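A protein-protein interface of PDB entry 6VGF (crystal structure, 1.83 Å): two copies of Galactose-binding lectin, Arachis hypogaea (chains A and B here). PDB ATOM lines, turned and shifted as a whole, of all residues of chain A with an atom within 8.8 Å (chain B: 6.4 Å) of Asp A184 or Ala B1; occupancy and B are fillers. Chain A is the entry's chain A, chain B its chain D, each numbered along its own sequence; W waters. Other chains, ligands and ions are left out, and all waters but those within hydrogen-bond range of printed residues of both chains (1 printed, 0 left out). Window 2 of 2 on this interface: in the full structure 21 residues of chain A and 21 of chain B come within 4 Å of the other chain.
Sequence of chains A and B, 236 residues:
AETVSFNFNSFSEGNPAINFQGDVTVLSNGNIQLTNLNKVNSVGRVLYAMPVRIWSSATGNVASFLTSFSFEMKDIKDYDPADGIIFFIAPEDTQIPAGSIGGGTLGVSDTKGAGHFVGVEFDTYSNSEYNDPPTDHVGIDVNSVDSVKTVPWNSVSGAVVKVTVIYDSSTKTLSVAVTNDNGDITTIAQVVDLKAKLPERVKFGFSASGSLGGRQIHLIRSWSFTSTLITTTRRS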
ATOM      1  N   TRP A 153      12.899  13.311   9.210  1.00  0.00           N
ATOM      2  CA  TRP A 153      14.319  13.052   9.008  1.00  0.00           C
ATOM      3  C   TRP A 153      14.630  13.443   7.559  1.00  0.00           C
ATOM      4  O   TRP A 153      13.726  13.900   6.838  1.00  0.00           O
ATOM      5  CB  TRP A 153      14.614  11.572   9.364  1.00  0.00           C
ATOM      6  CG  TRP A 153      16.003  11.068   9.074  1.00  0.00           C
ATOM      7  CD1 TRP A 153      17.165  11.431   9.699  1.00  0.00           C
ATOM      8  CD2 TRP A 153      16.352  10.044   8.135  1.00  0.00           C
ATOM      9  NE1 TRP A 153      18.219  10.715   9.181  1.00  0.00           N
ATOM     10  CE2 TRP A 153      17.750   9.870   8.204  1.00  0.00           C
ATOM     11  CE3 TRP A 153      15.616   9.272   7.219  1.00  0.00           C
ATOM     12  CZ2 TRP A 153      18.431   8.932   7.409  1.00  0.00           C
ATOM     13  CZ3 TRP A 153      16.292   8.358   6.416  1.00  0.00           C
ATOM     14  CH2 TRP A 153      17.680   8.192   6.521  1.00  0.00           C
ATOM     15  N   ASN A 154      15.891  13.392   7.164  1.00  0.00           N
ATOM     16  CA  ASN A 154      16.285  13.739   5.805  1.00  0.00           C
ATOM     17  C   ASN A 154      17.314  12.735   5.318  1.00  0.00           C
ATOM     18  O   ASN A 154      18.375  12.630   5.922  1.00  0.00           O
ATOM     19  CB  ASN A 154      16.829  15.187   5.748  1.00  0.00           C
ATOM     20  CG  ASN A 154      17.404  15.620   4.407  1.00  0.00           C
ATOM     21  OD1 ASN A 154      16.967  15.196   3.326  1.00  0.00           O
ATOM     22  ND2 ASN A 154      18.391  16.507   4.451  1.00  0.00           N
ATOM     23  N   VAL A 161      25.249   7.172   7.382  1.00  0.00           N
ATOM     24  CA  VAL A 161      24.365   7.405   8.532  1.00  0.00           C
ATOM     25  C   VAL A 161      24.698   6.381   9.625  1.00  0.00           C
ATOM     26  O   VAL A 161      24.862   5.198   9.325  1.00  0.00           O
ATOM     27  CB  VAL A 161      22.862   7.335   8.099  1.00  0.00           C
ATOM     28  CG1 VAL A 161      21.930   7.582   9.292  1.00  0.00           C
ATOM     29  CG2 VAL A 161      22.558   8.310   6.978  1.00  0.00           C
ATOM     30  N   LYS A 162      24.823   6.843  10.871  1.00  0.00           N
ATOM     31  CA  LYS A 162      25.100   6.010  12.048  1.00  0.00           C
ATOM     32  C   LYS A 162      23.845   5.916  12.899  1.00  0.00           C
ATOM     33  O   LYS A 162      23.153   6.916  13.106  1.00  0.00           O
ATOM     34  CB  LYS A 162      26.281   6.555  12.875  1.00  0.00           C
ATOM     35  CG  LYS A 162      27.607   6.447  12.152  1.00  0.00           C
ATOM     36  CD  LYS A 162      28.789   6.843  13.006  1.00  0.00           C
ATOM     37  CE  LYS A 162      30.058   6.659  12.220  1.00  0.00           C
ATOM     38  NZ  LYS A 162      30.273   7.717  11.187  1.00  0.00           N
ATOM     39  N   ALA A 177      18.746   6.542  18.118  1.00  0.00           N
ATOM     40  CA  ALA A 177      19.477   7.785  17.857  1.00  0.00           C
ATOM     41  C   ALA A 177      20.160   7.638  16.494  1.00  0.00           C
ATOM     42  O   ALA A 177      20.905   6.675  16.281  1.00  0.00           O
ATOM     43  CB  ALA A 177      20.484   8.091  18.966  1.00  0.00           C
ATOM     44  N   VAL A 178      19.873   8.576  15.585  1.00  0.00           N
ATOM     45  CA  VAL A 178      20.345   8.606  14.192  1.00  0.00           C
ATOM     46  C   VAL A 178      21.255   9.814  13.999  1.00  0.00           C
ATOM     47  O   VAL A 178      20.804  10.956  14.158  1.00  0.00           O
ATOM     48  CB  VAL A 178      19.162   8.616  13.184  1.00  0.00           C
ATOM     49  CG1 VAL A 178      19.652   8.433  11.750  1.00  0.00           C
ATOM     50  CG2 VAL A 178      18.119   7.560  13.540  1.00  0.00           C
ATOM     51  N   THR A 179      22.526   9.559  13.652  1.00  0.00           N
ATOM     52  CA  THR A 179      23.535  10.600  13.472  1.00  0.00           C
ATOM     53  C   THR A 179      23.732  10.848  11.993  1.00  0.00           C
ATOM     54  O   THR A 179      24.261   9.988  11.289  1.00  0.00           O
ATOM     55  CB  THR A 179      24.854  10.249  14.198  1.00  0.00           C
ATOM     56  OG1 THR A 179      24.584   9.988  15.574  1.00  0.00           O
ATOM     57  CG2 THR A 179      25.878  11.371  14.136  1.00  0.00           C
ATOM     58  N   ASN A 180      23.309  12.039  11.543  1.00  0.00           N
ATOM     59  CA  ASN A 180      23.397  12.533  10.167  1.00  0.00           C
ATOM     60  C   ASN A 180      24.810  13.060   9.843  1.00  0.00           C
ATOM     61  O   ASN A 180      25.630  13.264  10.751  1.00  0.00           O
ATOM     62  CB  ASN A 180      22.345  13.625   9.933  1.00  0.00           C
ATOM     63  CG  ASN A 180      20.929  13.111  10.102  1.00  0.00           C
ATOM     64  OD1 ASN A 180      20.465  12.270   9.307  1.00  0.00           O
ATOM     65  ND2 ASN A 180      20.236  13.572  11.168  1.00  0.00           N
ATOM     66  N   ASP A 181      25.081  13.243   8.528  1.00  0.00           N
ATOM     67  CA  ASP A 181      26.329  13.723   7.929  1.00  0.00           C
ATOM     68  C   ASP A 181      26.654  15.149   8.378  1.00  0.00           C
ATOM     69  O   ASP A 181      27.822  15.440   8.642  1.00  0.00           O
ATOM     70  CB  ASP A 181      26.187  13.655   6.372  1.00  0.00           C
ATOM     71  CG  ASP A 181      27.350  14.182   5.553  1.00  0.00           C
ATOM     72  OD1 ASP A 181      28.457  13.589   5.633  1.00  0.00           O
ATOM     73  OD2 ASP A 181      27.131  15.115   4.752  1.00  0.00           O
ATOM     74  N   ASN A 182      25.617  16.030   8.486  1.00  0.00           N
ATOM     75  CA  ASN A 182      25.749  17.435   8.883  1.00  0.00           C
ATOM     76  C   ASN A 182      26.000  17.600  10.411  1.00  0.00           C
ATOM     77  O   ASN A 182      26.085  18.741  10.899  1.00  0.00           O
ATOM     78  CB  ASN A 182      24.523  18.241   8.424  1.00  0.00           C
ATOM     79  CG  ASN A 182      23.302  18.245   9.317  1.00  0.00           C
ATOM     80  OD1 ASN A 182      22.650  19.281   9.464  1.00  0.00           O
ATOM     81  ND2 ASN A 182      22.920  17.104   9.899  1.00  0.00           N
ATOM     82  N   GLY A 183      26.122  16.477  11.131  1.00  0.00           N
ATOM     83  CA  GLY A 183      26.381  16.461  12.569  1.00  0.00           C
ATOM     84  C   GLY A 183      25.185  16.333  13.495  1.00  0.00           C
ATOM     85  O   GLY A 183      25.341  15.837  14.613  1.00  0.00           O
ATOM     86  N   ASP A 184      23.989  16.770  13.049  1.00  0.00           N
ATOM     87  CA  ASP A 184      22.744  16.734  13.831  1.00  0.00           C
ATOM     88  C   ASP A 184      22.305  15.320  14.197  1.00  0.00           C
ATOM     89  O   ASP A 184      22.545  14.381  13.439  1.00  0.00           O
ATOM     90  CB  ASP A 184      21.600  17.406  13.060  1.00  0.00           C
ATOM     91  CG  ASP A 184      21.681  18.916  12.887  1.00  0.00           C
ATOM     92  OD1 ASP A 184      22.766  19.496  13.157  1.00  0.00           O
ATOM     93  OD2 ASP A 184      20.678  19.512  12.418  1.00  0.00           O
ATOM     94  N   ILE A 185      21.648  15.180  15.358  1.00  0.00           N
ATOM     95  CA  ILE A 185      21.086  13.910  15.799  1.00  0.00           C
ATOM     96  C   ILE A 185      19.568  13.972  15.697  1.00  0.00           C
ATOM     97  O   ILE A 185      18.968  15.032  15.852  1.00  0.00           O
ATOM     98  CB  ILE A 185      21.553  13.397  17.196  1.00  0.00           C
ATOM     99  CG1 ILE A 185      21.467  14.457  18.275  1.00  0.00           C
ATOM    100  CG2 ILE A 185      22.930  12.765  17.117  1.00  0.00           C
ATOM    101  CD1 ILE A 185      20.449  14.121  19.229  1.00  0.00           C
ATOM    102  N   THR A 186      18.961  12.823  15.382  1.00  0.00           N
ATOM    103  CA  THR A 186      17.514  12.608  15.303  1.00  0.00           C
ATOM    104  C   THR A 186      17.214  11.461  16.260  1.00  0.00           C
ATOM    105  O   THR A 186      17.916  10.453  16.229  1.00  0.00           O
ATOM    106  CB  THR A 186      17.080  12.310  13.849  1.00  0.00           C
ATOM    107  OG1 THR A 186      17.498  13.372  12.989  1.00  0.00           O
ATOM    108  CG2 THR A 186      15.568  12.104  13.709  1.00  0.00           C
ATOM    109  N   THR A 187      16.194  11.599  17.106  1.00  0.00           N
ATOM    110  CA  THR A 187      15.838  10.507  18.011  1.00  0.00           C
ATOM    111  C   THR A 187      14.375  10.170  17.911  1.00  0.00           C
ATOM    112  O   THR A 187      13.543  11.026  17.570  1.00  0.00           O
ATOM    113  CB  THR A 187      16.203  10.781  19.496  1.00  0.00           C
ATOM    114  OG1 THR A 187      15.377  11.828  20.020  1.00  0.00           O
ATOM    115  CG2 THR A 187      17.693  11.056  19.727  1.00  0.00           C
ATOM    116  N   ALA B   1      18.770  23.596  12.739  1.00  0.00           N
ATOM    117  CA  ALA B   1      18.859  23.053  14.092  1.00  0.00           C
ATOM    118  C   ALA B   1      20.170  23.446  14.768  1.00  0.00           C
ATOM    119  O   ALA B   1      21.184  23.664  14.090  1.00  0.00           O
ATOM    120  CB  ALA B   1      18.719  21.535  14.061  1.00  0.00           C
ATOM    121  N   GLU B   2      20.141  23.530  16.111  1.00  0.00           N
ATOM    122  CA  GLU B   2      21.277  23.895  16.952  1.00  0.00           C
ATOM    123  C   GLU B   2      21.884  22.632  17.562  1.00  0.00           C
ATOM    124  O   GLU B   2      21.233  21.954  18.357  1.00  0.00           O
ATOM    125  CB  GLU B   2      20.821  24.870  18.029  1.00  0.00           C
ATOM    126  CG  GLU B   2      21.933  25.448  18.880  1.00  0.00           C
ATOM    127  CD  GLU B   2      21.398  26.488  19.842  1.00  0.00           C
ATOM    128  OE1 GLU B   2      20.993  27.575  19.370  1.00  0.00           O
ATOM    129  OE2 GLU B   2      21.331  26.199  21.058  1.00  0.00           O
ATOM    130  N   THR B   3      23.121  22.320  17.160  1.00  0.00           N
ATOM    131  CA  THR B   3      23.827  21.115  17.575  1.00  0.00           C
ATOM    132  C   THR B   3      25.146  21.444  18.287  1.00  0.00           C
ATOM    133  O   THR B   3      25.907  22.308  17.844  1.00  0.00           O
ATOM    134  CB  THR B   3      24.048  20.201  16.347  1.00  0.00           C
ATOM    135  OG1 THR B   3      22.784  19.718  15.901  1.00  0.00           O
ATOM    136  CG2 THR B   3      24.962  19.015  16.623  1.00  0.00           C
ATOM    137  N   THR B 226      26.704  14.432  21.420  1.00  0.00           N
ATOM    138  CA  THR B 226      25.980  15.191  20.412  1.00  0.00           C
ATOM    139  C   THR B 226      24.595  15.515  20.943  1.00  0.00           C
ATOM    140  O   THR B 226      23.854  14.611  21.313  1.00  0.00           O
ATOM    141  CB  THR B 226      25.862  14.508  19.007  1.00  0.00           C
ATOM    142  OG1 THR B 226      27.122  14.061  18.532  1.00  0.00           O
ATOM    143  CG2 THR B 226      25.247  15.442  17.979  1.00  0.00           C
ATOM    144  N   SER B 227      24.243  16.791  20.956  1.00  0.00           N
ATOM    145  CA  SER B 227      22.903  17.239  21.292  1.00  0.00           C
ATOM    146  C   SER B 227      22.381  18.042  20.113  1.00  0.00           C
ATOM    147  O   SER B 227      23.161  18.728  19.467  1.00  0.00           O
ATOM    148  CB  SER B 227      22.882  18.072  22.572  1.00  0.00           C
ATOM    149  OG  SER B 227      23.554  19.303  22.384  1.00  0.00           O
ATOM    150  N   THR B 228      21.087  17.967  19.851  1.00  0.00           N
ATOM    151  CA  THR B 228      20.447  18.694  18.754  1.00  0.00           C
ATOM    152  C   THR B 228      19.122  19.195  19.237  1.00  0.00           C
ATOM    153  O   THR B 228      18.288  18.421  19.702  1.00  0.00           O
ATOM    154  CB  THR B 228      20.329  17.833  17.473  1.00  0.00           C
ATOM    155  OG1 THR B 228      21.636  17.474  17.035  1.00  0.00           O
ATOM    156  CG2 THR B 228      19.598  18.557  16.314  1.00  0.00           C
ATOM    157  N   LEU B 229      18.953  20.515  19.147  1.00  0.00           N
ATOM    158  CA  LEU B 229      17.733  21.222  19.498  1.00  0.00           C
ATOM    159  C   LEU B 229      17.163  21.811  18.197  1.00  0.00           C
ATOM    160  O   LEU B 229      17.897  22.419  17.410  1.00  0.00           O
ATOM    161  CB  LEU B 229      18.000  22.292  20.583  1.00  0.00           C
ATOM    162  CG  LEU B 229      16.862  23.273  20.937  1.00  0.00           C
ATOM    163  CD1 LEU B 229      15.804  22.607  21.780  1.00  0.00           C
ATOM    164  CD2 LEU B 229      17.396  24.476  21.714  1.00  0.00           C
ATOM    165  N   ILE B 230      15.893  21.519  17.929  1.00  0.00           N
ATOM    166  CA  ILE B 230      15.177  22.018  16.744  1.00  0.00           C
ATOM    167  C   ILE B 230      14.868  23.496  16.993  1.00  0.00           C
ATOM    168  O   ILE B 230      14.355  23.838  18.053  1.00  0.00           O
ATOM    169  CB  ILE B 230      13.918  21.150  16.442  1.00  0.00           C
ATOM    170  CG1 ILE B 230      14.347  19.785  15.826  1.00  0.00           C
ATOM    171  CG2 ILE B 230      12.933  21.868  15.509  1.00  0.00           C
ATOM    172  CD1 ILE B 230      13.530  18.645  16.245  1.00  0.00           C
ATOM    173  N   THR B 231      15.249  24.370  16.040  1.00  0.00           N
ATOM    174  CA  THR B 231      15.074  25.811  16.187  1.00  0.00           C
ATOM    175  C   THR B 231      13.924  26.356  15.292  1.00  0.00           C
ATOM    176  O   THR B 231      13.879  27.563  15.024  1.00  0.00           O
ATOM    177  CB  THR B 231      16.409  26.561  15.966  1.00  0.00           C
ATOM    178  OG1 THR B 231      17.025  26.103  14.759  1.00  0.00           O
ATOM    179  CG2 THR B 231      17.368  26.445  17.171  1.00  0.00           C
HETATM  180  O   HOH W   1      27.737  15.023  15.633  1.00  0.00           O
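N of Asp A184 sits close to ND2 of Asn A182, 3.3 Å away.
The side-chain hydroxyl (OG1) of Thr B228 sits at hydrogen-bond distance from the side-chain hydroxyl (OG1) of Thr B3 (2.8 Å).
The side-chain amide nitrogen of Asn A180 is in hydrogen-bond range of the backbone carbonyl oxygen of Asp A184.
No position is printed for both chains.
Asp A184 touches just these residues of chain B: Ala B1, Thr B3 and Thr B228.
Printed residues of chain A within 4 Å of Thr B3: Gly A183 and Asp A184.
Of the printed residues of chain B, Ile A185 touches Thr B226 and Thr B228.
Printed residues of chain B within 4 Å of Gly A183: Thr B3 and Thr B226.
Ser B227 touches none of the printed residues of chain A.
Val A178 touches none of the printed residues of chain B.
The nearest residue of chain A that does not touch Ala B1 is Asn A182 (6.5 Å).
The nearest printed residue of chain A that does not touch Thr B228 is Gly A183 (4.7 Å).
Gly A183 touches Thr B3 (O to CG2, 3.8 Å).
Gly A183 touches Thr B226 (O to CG2, 3.4 Å).
CB of Ala B1 touches OD2 of Asp A184, at 3.3 Å.
Thr B228 touches Asp A184.
Ile A185 touches Thr B226.
Water W1 bridges O of Gly A183 and OG1 of Thr B226.
The side-chain hydroxyl (OG1) of Thr B228 sits at hydrogen-bond distance from the backbone NH (N) of Ile A185, at 2.8 Å.
OD1 of Asp A184 is in hydrogen-bond range of OG1 of Thr B3 (2.8 Å).
Printed residues of chain B that touch a printed residue of chain A: Ala B1, Thr B3, Thr B226 and Thr B228.
Of the 15 printed residues of chain A, 3 touch a printed residue of chain B.
Printed residues of chain A that touch a printed residue of chain B: Gly A183, Asp A184 and Ile A185.
Hydrophobic or aromatic side chains of chain A that line the printed part of chain B: Ile A185.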
